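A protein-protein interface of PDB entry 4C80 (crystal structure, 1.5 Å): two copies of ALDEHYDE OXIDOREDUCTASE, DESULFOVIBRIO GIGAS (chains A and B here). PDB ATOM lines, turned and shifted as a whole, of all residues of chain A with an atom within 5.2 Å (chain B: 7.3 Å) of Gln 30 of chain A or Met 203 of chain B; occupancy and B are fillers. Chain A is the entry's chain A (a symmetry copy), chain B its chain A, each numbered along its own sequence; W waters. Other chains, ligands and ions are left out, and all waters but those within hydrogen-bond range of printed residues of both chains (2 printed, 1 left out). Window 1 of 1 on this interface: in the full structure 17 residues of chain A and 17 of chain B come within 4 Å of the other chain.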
ATOM      1  N   MET A   1      -0.620 -29.773 -19.419  1.00  0.00           N
ATOM      2  CA  MET A   1       0.317 -29.737 -20.585  1.00  0.00           C
ATOM      3  C   MET A   1       1.693 -30.221 -20.150  1.00  0.00           C
ATOM      4  O   MET A   1       2.057 -30.131 -18.968  1.00  0.00           O
ATOM      5  CB  MET A   1       0.393 -28.294 -21.120  1.00  0.00           C
ATOM      6  CG  MET A   1       1.576 -28.012 -22.046  1.00  0.00           C
ATOM      7  SD  MET A   1       1.393 -26.418 -22.861  1.00  0.00           S
ATOM      8  CE  MET A   1       0.282 -26.832 -24.188  1.00  0.00           C
ATOM      9  N   PHE A  16       5.231 -28.909 -27.088  1.00  0.00           N
ATOM     10  CA  PHE A  16       4.322 -28.651 -25.988  1.00  0.00           C
ATOM     11  C   PHE A  16       2.972 -29.226 -26.325  1.00  0.00           C
ATOM     12  O   PHE A  16       2.326 -28.794 -27.278  1.00  0.00           O
ATOM     13  CB  PHE A  16       4.272 -27.152 -25.732  1.00  0.00           C
ATOM     14  CG  PHE A  16       5.587 -26.631 -25.238  1.00  0.00           C
ATOM     15  CD1 PHE A  16       6.576 -26.266 -26.132  1.00  0.00           C
ATOM     16  CD2 PHE A  16       5.884 -26.655 -23.885  1.00  0.00           C
ATOM     17  CE1 PHE A  16       7.828 -25.901 -25.688  1.00  0.00           C
ATOM     18  CE2 PHE A  16       7.126 -26.254 -23.443  1.00  0.00           C
ATOM     19  CZ  PHE A  16       8.091 -25.874 -24.339  1.00  0.00           C
ATOM     20  N   VAL A  17       2.577 -30.221 -25.542  1.00  0.00           N
ATOM     21  CA  VAL A  17       1.428 -31.043 -25.876  1.00  0.00           C
ATOM     22  C   VAL A  17       0.563 -31.372 -24.667  1.00  0.00           C
ATOM     23  O   VAL A  17       1.025 -31.337 -23.535  1.00  0.00           O
ATOM     24  CB  VAL A  17       1.852 -32.381 -26.538  1.00  0.00           C
ATOM     25  CG1 VAL A  17       2.477 -32.121 -27.915  1.00  0.00           C
ATOM     26  CG2 VAL A  17       2.768 -33.192 -25.624  1.00  0.00           C
ATOM     27  N   ASP A  25      -2.825 -35.697 -34.615  1.00  0.00           N
ATOM     28  CA  ASP A  25      -3.182 -34.274 -34.503  1.00  0.00           C
ATOM     29  C   ASP A  25      -1.965 -33.420 -34.218  1.00  0.00           C
ATOM     30  O   ASP A  25      -1.790 -32.345 -34.779  1.00  0.00           O
ATOM     31  CB  ASP A  25      -4.230 -34.059 -33.413  1.00  0.00           C
ATOM     32  CG  ASP A  25      -5.600 -34.615 -33.783  1.00  0.00           C
ATOM     33  OD1 ASP A  25      -5.946 -34.643 -34.983  1.00  0.00           O
ATOM     34  OD2 ASP A  25      -6.344 -35.015 -32.869  1.00  0.00           O
ATOM     35  N   VAL A  26      -1.117 -33.877 -33.312  1.00  0.00           N
ATOM     36  CA  VAL A  26       0.105 -33.123 -33.004  1.00  0.00           C
ATOM     37  C   VAL A  26       0.955 -32.957 -34.264  1.00  0.00           C
ATOM     38  O   VAL A  26       1.383 -31.853 -34.598  1.00  0.00           O
ATOM     39  CB  VAL A  26       0.900 -33.789 -31.882  1.00  0.00           C
ATOM     40  CG1 VAL A  26       2.230 -33.077 -31.669  1.00  0.00           C
ATOM     41  CG2 VAL A  26       0.056 -33.794 -30.596  1.00  0.00           C
ATOM     42  N   LEU A  27       1.203 -34.058 -34.971  1.00  0.00           N
ATOM     43  CA  LEU A  27       2.050 -34.002 -36.162  1.00  0.00           C
ATOM     44  C   LEU A  27       1.424 -33.132 -37.260  1.00  0.00           C
ATOM     45  O   LEU A  27       2.098 -32.276 -37.819  1.00  0.00           O
ATOM     46  CB  LEU A  27       2.355 -35.402 -36.685  1.00  0.00           C
ATOM     47  CG  LEU A  27       3.165 -36.307 -35.749  1.00  0.00           C
ATOM     48  CD1 LEU A  27       3.265 -37.718 -36.312  1.00  0.00           C
ATOM     49  CD2 LEU A  27       4.552 -35.755 -35.480  1.00  0.00           C
ATOM     50  N   ARG A  28       0.136 -33.335 -37.536  1.00  0.00           N
ATOM     51  CA  ARG A  28      -0.517 -32.598 -38.629  1.00  0.00           C
ATOM     52  C   ARG A  28      -0.755 -31.132 -38.291  1.00  0.00           C
ATOM     53  O   ARG A  28      -0.457 -30.260 -39.089  1.00  0.00           O
ATOM     54  CB  ARG A  28      -1.864 -33.233 -39.012  1.00  0.00           C
ATOM     55  CG  ARG A  28      -1.751 -34.584 -39.699  1.00  0.00           C
ATOM     56  CD  ARG A  28      -3.109 -35.271 -39.915  1.00  0.00           C
ATOM     57  NE  ARG A  28      -4.038 -34.441 -40.681  1.00  0.00           N
ATOM     58  CZ  ARG A  28      -3.968 -34.235 -41.997  1.00  0.00           C
ATOM     59  NH1 ARG A  28      -3.022 -34.811 -42.730  1.00  0.00           N
ATOM     60  NH2 ARG A  28      -4.844 -33.411 -42.586  1.00  0.00           N
ATOM     61  N   GLN A  29      -1.332 -30.868 -37.119  1.00  0.00           N
ATOM     62  CA  GLN A  29      -1.806 -29.526 -36.762  1.00  0.00           C
ATOM     63  C   GLN A  29      -0.717 -28.684 -36.103  1.00  0.00           C
ATOM     64  O   GLN A  29      -0.511 -27.532 -36.498  1.00  0.00           O
ATOM     65  CB  GLN A  29      -3.015 -29.629 -35.852  1.00  0.00           C
ATOM     66  CG  GLN A  29      -4.147 -30.397 -36.492  1.00  0.00           C
ATOM     67  CD  GLN A  29      -5.428 -30.323 -35.720  1.00  0.00           C
ATOM     68  OE1 GLN A  29      -5.805 -29.264 -35.222  1.00  0.00           O
ATOM     69  NE2 GLN A  29      -6.132 -31.446 -35.649  1.00  0.00           N
ATOM     70  N   GLN A  30      -0.013 -29.233 -35.113  1.00  0.00           N
ATOM     71  CA  GLN A  30       1.013 -28.454 -34.408  1.00  0.00           C
ATOM     72  C   GLN A  30       2.300 -28.325 -35.230  1.00  0.00           C
ATOM     73  O   GLN A  30       2.918 -27.241 -35.254  1.00  0.00           O
ATOM     74  CB  GLN A  30       1.304 -29.022 -33.018  1.00  0.00           C
ATOM     75  CG  GLN A  30       0.114 -28.883 -32.088  1.00  0.00           C
ATOM     76  CD  GLN A  30       0.324 -29.446 -30.705  1.00  0.00           C
ATOM     77  OE1 GLN A  30      -0.425 -30.337 -30.269  1.00  0.00           O
ATOM     78  NE2 GLN A  30       1.307 -28.920 -29.980  1.00  0.00           N
ATOM     79  N   LEU A  31       2.685 -29.402 -35.918  1.00  0.00           N
ATOM     80  CA  LEU A  31       3.931 -29.399 -36.686  1.00  0.00           C
ATOM     81  C   LEU A  31       3.772 -29.248 -38.193  1.00  0.00           C
ATOM     82  O   LEU A  31       4.760 -29.158 -38.899  1.00  0.00           O
ATOM     83  CB  LEU A  31       4.772 -30.637 -36.360  1.00  0.00           C
ATOM     84  CG  LEU A  31       5.146 -30.861 -34.883  1.00  0.00           C
ATOM     85  CD1 LEU A  31       6.078 -32.058 -34.722  1.00  0.00           C
ATOM     86  CD2 LEU A  31       5.760 -29.595 -34.288  1.00  0.00           C
ATOM     87  N   GLY A  32       2.539 -29.245 -38.687  1.00  0.00           N
ATOM     88  CA  GLY A  32       2.292 -29.038 -40.118  1.00  0.00           C
ATOM     89  C   GLY A  32       2.671 -30.217 -41.020  1.00  0.00           C
ATOM     90  O   GLY A  32       2.803 -30.060 -42.238  1.00  0.00           O
ATOM     91  N   GLY B  32       3.378 -23.264 -41.821  1.00  0.00           N
ATOM     92  CA  GLY B  32       4.283 -23.770 -40.782  1.00  0.00           C
ATOM     93  C   GLY B  32       5.762 -23.433 -40.989  1.00  0.00           C
ATOM     94  O   GLY B  32       6.639 -24.047 -40.374  1.00  0.00           O
ATOM     95  N   THR B  34       8.135 -21.508 -39.924  1.00  0.00           N
ATOM     96  CA  THR B  34       8.562 -20.629 -38.839  1.00  0.00           C
ATOM     97  C   THR B  34      10.020 -20.198 -38.948  1.00  0.00           C
ATOM     98  O   THR B  34      10.481 -19.389 -38.153  1.00  0.00           O
ATOM     99  CB  THR B  34       8.284 -21.274 -37.463  1.00  0.00           C
ATOM    100  OG1 THR B  34       8.935 -22.554 -37.388  1.00  0.00           O
ATOM    101  CG2 THR B  34       6.784 -21.439 -37.259  1.00  0.00           C
ATOM    102  N   GLY B 196      10.421 -18.184 -28.879  1.00  0.00           N
ATOM    103  CA  GLY B 196       9.143 -18.187 -28.194  1.00  0.00           C
ATOM    104  C   GLY B 196       7.903 -17.984 -29.054  1.00  0.00           C
ATOM    105  O   GLY B 196       6.859 -18.602 -28.816  1.00  0.00           O
ATOM    106  N   ASP B 198       7.652 -18.755 -32.269  1.00  0.00           N
ATOM    107  CA  ASP B 198       7.589 -19.987 -33.066  1.00  0.00           C
ATOM    108  C   ASP B 198       6.871 -21.085 -32.238  1.00  0.00           C
ATOM    109  O   ASP B 198       5.979 -21.787 -32.740  1.00  0.00           O
ATOM    110  CB  ASP B 198       8.979 -20.477 -33.459  1.00  0.00           C
ATOM    111  CG  ASP B 198       9.828 -19.417 -34.156  1.00  0.00           C
ATOM    112  OD1 ASP B 198       9.232 -18.630 -34.922  1.00  0.00           O
ATOM    113  OD2 ASP B 198      11.065 -19.418 -33.976  1.00  0.00           O
ATOM    114  N   LEU B 199       7.268 -21.226 -30.978  1.00  0.00           N
ATOM    115  CA  LEU B 199       6.648 -22.189 -30.062  1.00  0.00           C
ATOM    116  C   LEU B 199       5.146 -21.908 -29.911  1.00  0.00           C
ATOM    117  O   LEU B 199       4.323 -22.829 -29.915  1.00  0.00           O
ATOM    118  CB  LEU B 199       7.378 -22.192 -28.720  1.00  0.00           C
ATOM    119  CG  LEU B 199       8.819 -22.712 -28.799  1.00  0.00           C
ATOM    120  CD1 LEU B 199       9.561 -22.441 -27.504  1.00  0.00           C
ATOM    121  CD2 LEU B 199       8.860 -24.197 -29.151  1.00  0.00           C
ATOM    122  N   GLY B 200       4.773 -20.636 -29.813  1.00  0.00           N
ATOM    123  CA  GLY B 200       3.369 -20.251 -29.744  1.00  0.00           C
ATOM    124  C   GLY B 200       2.549 -20.798 -30.897  1.00  0.00           C
ATOM    125  O   GLY B 200       1.421 -21.237 -30.697  1.00  0.00           O
ATOM    126  N   LEU B 201       3.111 -20.783 -32.104  1.00  0.00           N
ATOM    127  CA  LEU B 201       2.395 -21.270 -33.280  1.00  0.00           C
ATOM    128  C   LEU B 201       2.237 -22.791 -33.264  1.00  0.00           C
ATOM    129  O   LEU B 201       1.373 -23.332 -33.947  1.00  0.00           O
ATOM    130  CB  LEU B 201       3.110 -20.813 -34.553  1.00  0.00           C
ATOM    131  CG  LEU B 201       3.011 -19.322 -34.865  1.00  0.00           C
ATOM    132  CD1 LEU B 201       3.631 -19.051 -36.224  1.00  0.00           C
ATOM    133  CD2 LEU B 201       1.595 -18.802 -34.830  1.00  0.00           C
ATOM    134  N   LYS B 202       3.094 -23.465 -32.504  1.00  0.00           N
ATOM    135  CA  LYS B 202       3.158 -24.923 -32.464  1.00  0.00           C
ATOM    136  C   LYS B 202       2.554 -25.495 -31.180  1.00  0.00           C
ATOM    137  O   LYS B 202       2.711 -26.677 -30.885  1.00  0.00           O
ATOM    138  CB  LYS B 202       4.620 -25.377 -32.660  1.00  0.00           C
ATOM    139  CG  LYS B 202       5.211 -24.883 -33.989  1.00  0.00           C
ATOM    140  CD  LYS B 202       6.665 -25.273 -34.174  1.00  0.00           C
ATOM    141  CE  LYS B 202       7.230 -24.601 -35.412  1.00  0.00           C
ATOM    142  NZ  LYS B 202       8.530 -25.208 -35.814  1.00  0.00           N
ATOM    143  N   MET B 203       1.870 -24.650 -30.419  1.00  0.00           N
ATOM    144  CA  MET B 203       1.198 -25.082 -29.219  1.00  0.00           C
ATOM    145  C   MET B 203      -0.186 -25.584 -29.620  1.00  0.00           C
ATOM    146  O   MET B 203      -0.697 -25.302 -30.718  1.00  0.00           O
ATOM    147  CB  MET B 203       1.110 -23.924 -28.201  1.00  0.00           C
ATOM    148  CG  MET B 203       2.423 -23.693 -27.463  1.00  0.00           C
ATOM    149  SD  MET B 203       2.483 -22.252 -26.377  1.00  0.00           S
ATOM    150  CE  MET B 203       1.632 -22.861 -24.934  1.00  0.00           C
ATOM    151  N   PRO B 204      -0.812 -26.322 -28.732  1.00  0.00           N
ATOM    152  CA  PRO B 204      -2.093 -26.930 -29.129  1.00  0.00           C
ATOM    153  C   PRO B 204      -3.268 -25.971 -29.159  1.00  0.00           C
ATOM    154  O   PRO B 204      -3.217 -24.929 -28.527  1.00  0.00           O
ATOM    155  CB  PRO B 204      -2.304 -28.016 -28.095  1.00  0.00           C
ATOM    156  CG  PRO B 204      -1.475 -27.669 -26.930  1.00  0.00           C
ATOM    157  CD  PRO B 204      -0.360 -26.749 -27.405  1.00  0.00           C
ATOM    158  N   ALA B 205      -4.326 -26.345 -29.881  1.00  0.00           N
ATOM    159  CA  ALA B 205      -5.564 -25.569 -29.895  1.00  0.00           C
ATOM    160  C   ALA B 205      -6.034 -25.472 -28.457  1.00  0.00           C
ATOM    161  O   ALA B 205      -5.713 -26.310 -27.614  1.00  0.00           O
ATOM    162  CB  ALA B 205      -6.626 -26.234 -30.762  1.00  0.00           C
ATOM    163  N   GLY B 206      -6.753 -24.441 -28.117  1.00  0.00           N
ATOM    164  CA  GLY B 206      -7.052 -24.319 -26.679  1.00  0.00           C
ATOM    165  C   GLY B 206      -5.959 -23.663 -25.837  1.00  0.00           C
ATOM    166  O   GLY B 206      -6.223 -23.267 -24.719  1.00  0.00           O
ATOM    167  N   THR B 207      -4.733 -23.560 -26.346  1.00  0.00           N
ATOM    168  CA  THR B 207      -3.826 -22.515 -25.839  1.00  0.00           C
ATOM    169  C   THR B 207      -4.529 -21.164 -25.997  1.00  0.00           C
ATOM    170  O   THR B 207      -5.110 -20.873 -27.045  1.00  0.00           O
ATOM    171  CB  THR B 207      -2.494 -22.499 -26.590  1.00  0.00           C
ATOM    172  OG1 THR B 207      -1.818 -23.744 -26.380  1.00  0.00           O
ATOM    173  CG2 THR B 207      -1.576 -21.354 -26.120  1.00  0.00           C
ATOM    174  N   LEU B 208      -4.517 -20.376 -24.938  1.00  0.00           N
ATOM    175  CA  LEU B 208      -5.067 -19.034 -24.977  1.00  0.00           C
ATOM    176  C   LEU B 208      -3.950 -18.032 -25.308  1.00  0.00           C
ATOM    177  O   LEU B 208      -2.855 -18.135 -24.784  1.00  0.00           O
ATOM    178  CB  LEU B 208      -5.726 -18.691 -23.643  1.00  0.00           C
ATOM    179  CG  LEU B 208      -6.982 -19.501 -23.323  1.00  0.00           C
ATOM    180  CD1 LEU B 208      -7.422 -19.275 -21.880  1.00  0.00           C
ATOM    181  CD2 LEU B 208      -8.108 -19.142 -24.276  1.00  0.00           C
ATOM    182  N   HIS B 209      -4.271 -17.048 -26.134  1.00  0.00           N
ATOM    183  CA  HIS B 209      -3.344 -15.998 -26.539  1.00  0.00           C
ATOM    184  C   HIS B 209      -3.719 -14.743 -25.817  1.00  0.00           C
ATOM    185  O   HIS B 209      -4.910 -14.401 -25.717  1.00  0.00           O
ATOM    186  CB  HIS B 209      -3.359 -15.842 -28.061  1.00  0.00           C
ATOM    187  CG  HIS B 209      -2.774 -17.033 -28.749  1.00  0.00           C
ATOM    188  ND1 HIS B 209      -3.518 -18.138 -29.114  1.00  0.00           N
ATOM    189  CD2 HIS B 209      -1.495 -17.329 -29.060  1.00  0.00           C
ATOM    190  CE1 HIS B 209      -2.717 -19.044 -29.641  1.00  0.00           C
ATOM    191  NE2 HIS B 209      -1.489 -18.576 -29.622  1.00  0.00           N
ATOM    192  N   ALA B 373       6.667 -14.868 -24.081  1.00  0.00           N
ATOM    193  CA  ALA B 373       6.700 -15.901 -23.057  1.00  0.00           C
ATOM    194  C   ALA B 373       5.406 -16.682 -23.092  1.00  0.00           C
ATOM    195  O   ALA B 373       4.381 -16.216 -23.640  1.00  0.00           O
ATOM    196  CB  ALA B 373       6.869 -15.278 -21.679  1.00  0.00           C
ATOM    197  N   PHE B 374       5.437 -17.844 -22.454  1.00  0.00           N
ATOM    198  CA  PHE B 374       4.236 -18.657 -22.277  1.00  0.00           C
ATOM    199  C   PHE B 374       4.283 -19.413 -20.982  1.00  0.00           C
ATOM    200  O   PHE B 374       5.348 -19.541 -20.388  1.00  0.00           O
ATOM    201  CB  PHE B 374       3.952 -19.564 -23.492  1.00  0.00           C
ATOM    202  CG  PHE B 374       5.028 -20.568 -23.832  1.00  0.00           C
ATOM    203  CD1 PHE B 374       6.034 -20.245 -24.715  1.00  0.00           C
ATOM    204  CD2 PHE B 374       4.985 -21.866 -23.343  1.00  0.00           C
ATOM    205  CE1 PHE B 374       6.969 -21.178 -25.102  1.00  0.00           C
ATOM    206  CE2 PHE B 374       5.941 -22.794 -23.701  1.00  0.00           C
ATOM    207  CZ  PHE B 374       6.938 -22.446 -24.593  1.00  0.00           C
ATOM    208  N   ALA B 375       3.132 -19.906 -20.536  1.00  0.00           N
ATOM    209  CA  ALA B 375       3.046 -20.635 -19.282  1.00  0.00           C
ATOM    210  C   ALA B 375       1.919 -21.632 -19.365  1.00  0.00           C
ATOM    211  O   ALA B 375       0.998 -21.490 -20.178  1.00  0.00           O
ATOM    212  CB  ALA B 375       2.813 -19.700 -18.120  1.00  0.00           C
ATOM    213  N   TYR B 376       1.988 -22.630 -18.504  1.00  0.00           N
ATOM    214  CA  TYR B 376       0.930 -23.658 -18.446  1.00  0.00           C
ATOM    215  C   TYR B 376       0.983 -24.343 -17.094  1.00  0.00           C
ATOM    216  O   TYR B 376       1.991 -24.277 -16.389  1.00  0.00           O
ATOM    217  CB  TYR B 376       1.097 -24.683 -19.584  1.00  0.00           C
ATOM    218  CG  TYR B 376       2.455 -25.310 -19.658  1.00  0.00           C
ATOM    219  CD1 TYR B 376       3.491 -24.726 -20.409  1.00  0.00           C
ATOM    220  CD2 TYR B 376       2.752 -26.472 -18.950  1.00  0.00           C
ATOM    221  CE1 TYR B 376       4.755 -25.302 -20.446  1.00  0.00           C
ATOM    222  CE2 TYR B 376       4.023 -27.036 -18.977  1.00  0.00           C
ATOM    223  CZ  TYR B 376       5.026 -26.436 -19.734  1.00  0.00           C
ATOM    224  OH  TYR B 376       6.293 -26.974 -19.768  1.00  0.00           O
ATOM    225  N   ARG B 442      -5.300 -23.032 -18.212  1.00  0.00           N
ATOM    226  CA  ARG B 442      -5.044 -23.351 -19.615  1.00  0.00           C
ATOM    227  C   ARG B 442      -3.642 -22.850 -19.971  1.00  0.00           C
ATOM    228  O   ARG B 442      -3.133 -21.913 -19.320  1.00  0.00           O
ATOM    229  CB  ARG B 442      -6.060 -22.636 -20.514  1.00  0.00           C
ATOM    230  CG  ARG B 442      -7.529 -22.964 -20.237  1.00  0.00           C
ATOM    231  CD  ARG B 442      -8.143 -23.898 -21.232  1.00  0.00           C
ATOM    232  NE  ARG B 442      -8.186 -23.426 -22.617  1.00  0.00           N
ATOM    233  CZ  ARG B 442      -9.252 -22.955 -23.267  1.00  0.00           C
ATOM    234  NH1 ARG B 442     -10.436 -22.796 -22.677  1.00  0.00           N
ATOM    235  NH2 ARG B 442      -9.118 -22.619 -24.544  1.00  0.00           N
ATOM    236  N   PRO B 443      -3.020 -23.450 -20.997  1.00  0.00           N
ATOM    237  CA  PRO B 443      -1.809 -22.838 -21.529  1.00  0.00           C
ATOM    238  C   PRO B 443      -2.102 -21.439 -22.070  1.00  0.00           C
ATOM    239  O   PRO B 443      -3.173 -21.186 -22.676  1.00  0.00           O
ATOM    240  CB  PRO B 443      -1.383 -23.784 -22.666  1.00  0.00           C
ATOM    241  CG  PRO B 443      -2.140 -25.050 -22.415  1.00  0.00           C
ATOM    242  CD  PRO B 443      -3.422 -24.625 -21.785  1.00  0.00           C
ATOM    243  N   VAL B 444      -1.146 -20.543 -21.850  1.00  0.00           N
ATOM    244  CA  VAL B 444      -1.271 -19.175 -22.289  1.00  0.00           C
ATOM    245  C   VAL B 444       0.014 -18.717 -22.943  1.00  0.00           C
ATOM    246  O   VAL B 444       1.100 -19.133 -22.532  1.00  0.00           O
ATOM    247  CB  VAL B 444      -1.630 -18.227 -21.119  1.00  0.00           C
ATOM    248  CG1 VAL B 444      -2.935 -18.667 -20.451  1.00  0.00           C
ATOM    249  CG2 VAL B 444      -0.495 -18.103 -20.103  1.00  0.00           C
ATOM    250  N   HIS B 445      -0.119 -17.831 -23.934  1.00  0.00           N
ATOM    251  CA  HIS B 445       1.026 -17.328 -24.699  1.00  0.00           C
ATOM    252  C   HIS B 445       0.864 -15.825 -24.912  1.00  0.00           C
ATOM    253  O   HIS B 445      -0.215 -15.363 -25.310  1.00  0.00           O
ATOM    254  CB  HIS B 445       1.117 -18.058 -26.042  1.00  0.00           C
ATOM    255  CG  HIS B 445       2.366 -17.761 -26.812  1.00  0.00           C
ATOM    256  ND1 HIS B 445       2.491 -16.656 -27.622  1.00  0.00           N
ATOM    257  CD2 HIS B 445       3.541 -18.431 -26.905  1.00  0.00           C
ATOM    258  CE1 HIS B 445       3.692 -16.656 -28.186  1.00  0.00           C
ATOM    259  NE2 HIS B 445       4.352 -17.725 -27.768  1.00  0.00           N
HETATM  260  O   HOH W   1       6.031 -26.012 -38.502  1.00  0.00           O
HETATM  261  O   HOH W   2       5.091 -27.568 -29.632  1.00  0.00           O
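The side-chain amide nitrogen of Gln 30 of chain A sits at hydrogen-bond distance from the backbone carbonyl oxygen of Lys 202 of chain B (2.8 Å).
The side-chain hydroxyl (OG1) of Thr 34 of chain B is in hydrogen-bond range of the side-chain amino group (NZ) of Lys 202 of chain B (3.1 Å). The backbone carbonyl oxygen (O) of Pro 204 of chain B is in hydrogen-bond range of the side-chain hydroxyl (OG1) of Thr 207 of chain B, 2.8 Å away. The backbone carbonyl oxygen of Pro 443 of chain B lies within hydrogen-bond range of the backbone NH of Leu 208 of chain B (2.8 Å). NE2 of Gln 30 of chain A lies within hydrogen-bond range of O of Phe 16 of chain A (2.9 Å).
Met 1 of chain A touches Pro 204 of chain B (CE to CD, 3.3 Å). Tyr 376 of chain B touches Met 1 of chain A. CE of Met 1 of chain A touches CG of Pro 443 of chain B (3.5 Å). CD2 of Leu 199 of chain B touches CE1 of Phe 16 of chain A (3.995 Å). Phe 16 of chain A touches Pro 204 of chain B. Phe 16 of chain A touches Phe 374 of chain B. Phe 16 of chain A touches Tyr 376 of chain B. Gln 30 of chain A touches Met 203 of chain B (NE2 to C, 3.7 Å). Pro 204 of chain B touches Gln 30 of chain A.
Of the printed residues of chain B, Met 1 of chain A touches Pro 204 (3.3 Å), Tyr 376 (3.6 Å) and Pro 443 (3.5 Å). Gln 30 of chain A touches three residues of chain B. Met 203 of chain B touches just one residue of chain A: Gln 30. Of the printed residues of chain A, Pro 204 of chain B touches Met 1, Phe 16 and Gln 30. Of the printed residues of chain A, Tyr 376 of chain B touches Met 1 and Phe 16. The nearest residue of chain B that does not touch Gln 30 of chain A is Leu 201 of chain B (4.4 Å). The nearest residue of chain A that does not touch Met 203 of chain B is Met 1 of chain A (4.1 Å).
Of the 11 printed residues of chain A, 3 touch a printed residue of chain B. Printed residues of chain A that touch a printed residue of chain B: Met 1, Phe 16 and Gln 30. Hydrophobic or aromatic side chains of chain A that line the printed part of chain B: Met 1 and Phe 16. Of the 23 printed residues of chain B, 7 touch a printed residue of chain A. Printed residues of chain B that touch a printed residue of chain A: Leu 199, Lys 202, Met 203, Pro 204, Phe 374, Tyr 376 and Pro 443. Among the printed residues, no Asp or Glu carboxylate lies within 4 Å of a Lys or Arg side-chain nitrogen of the other chain.
1 position is printed for both chains. Of the 10 pairs that touch across the chains among the printed residues, none has its exchanged pair printed and touching as well.
Water W1 lies within hydrogen-bond range of O of Gly 32 of chain B and O of Leu 31 of chain A. Water W2 bridges the backbone carbonyl oxygen (O) of Lys 202 of chain B and the backbone NH (N) of Phe 16 of chain A.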
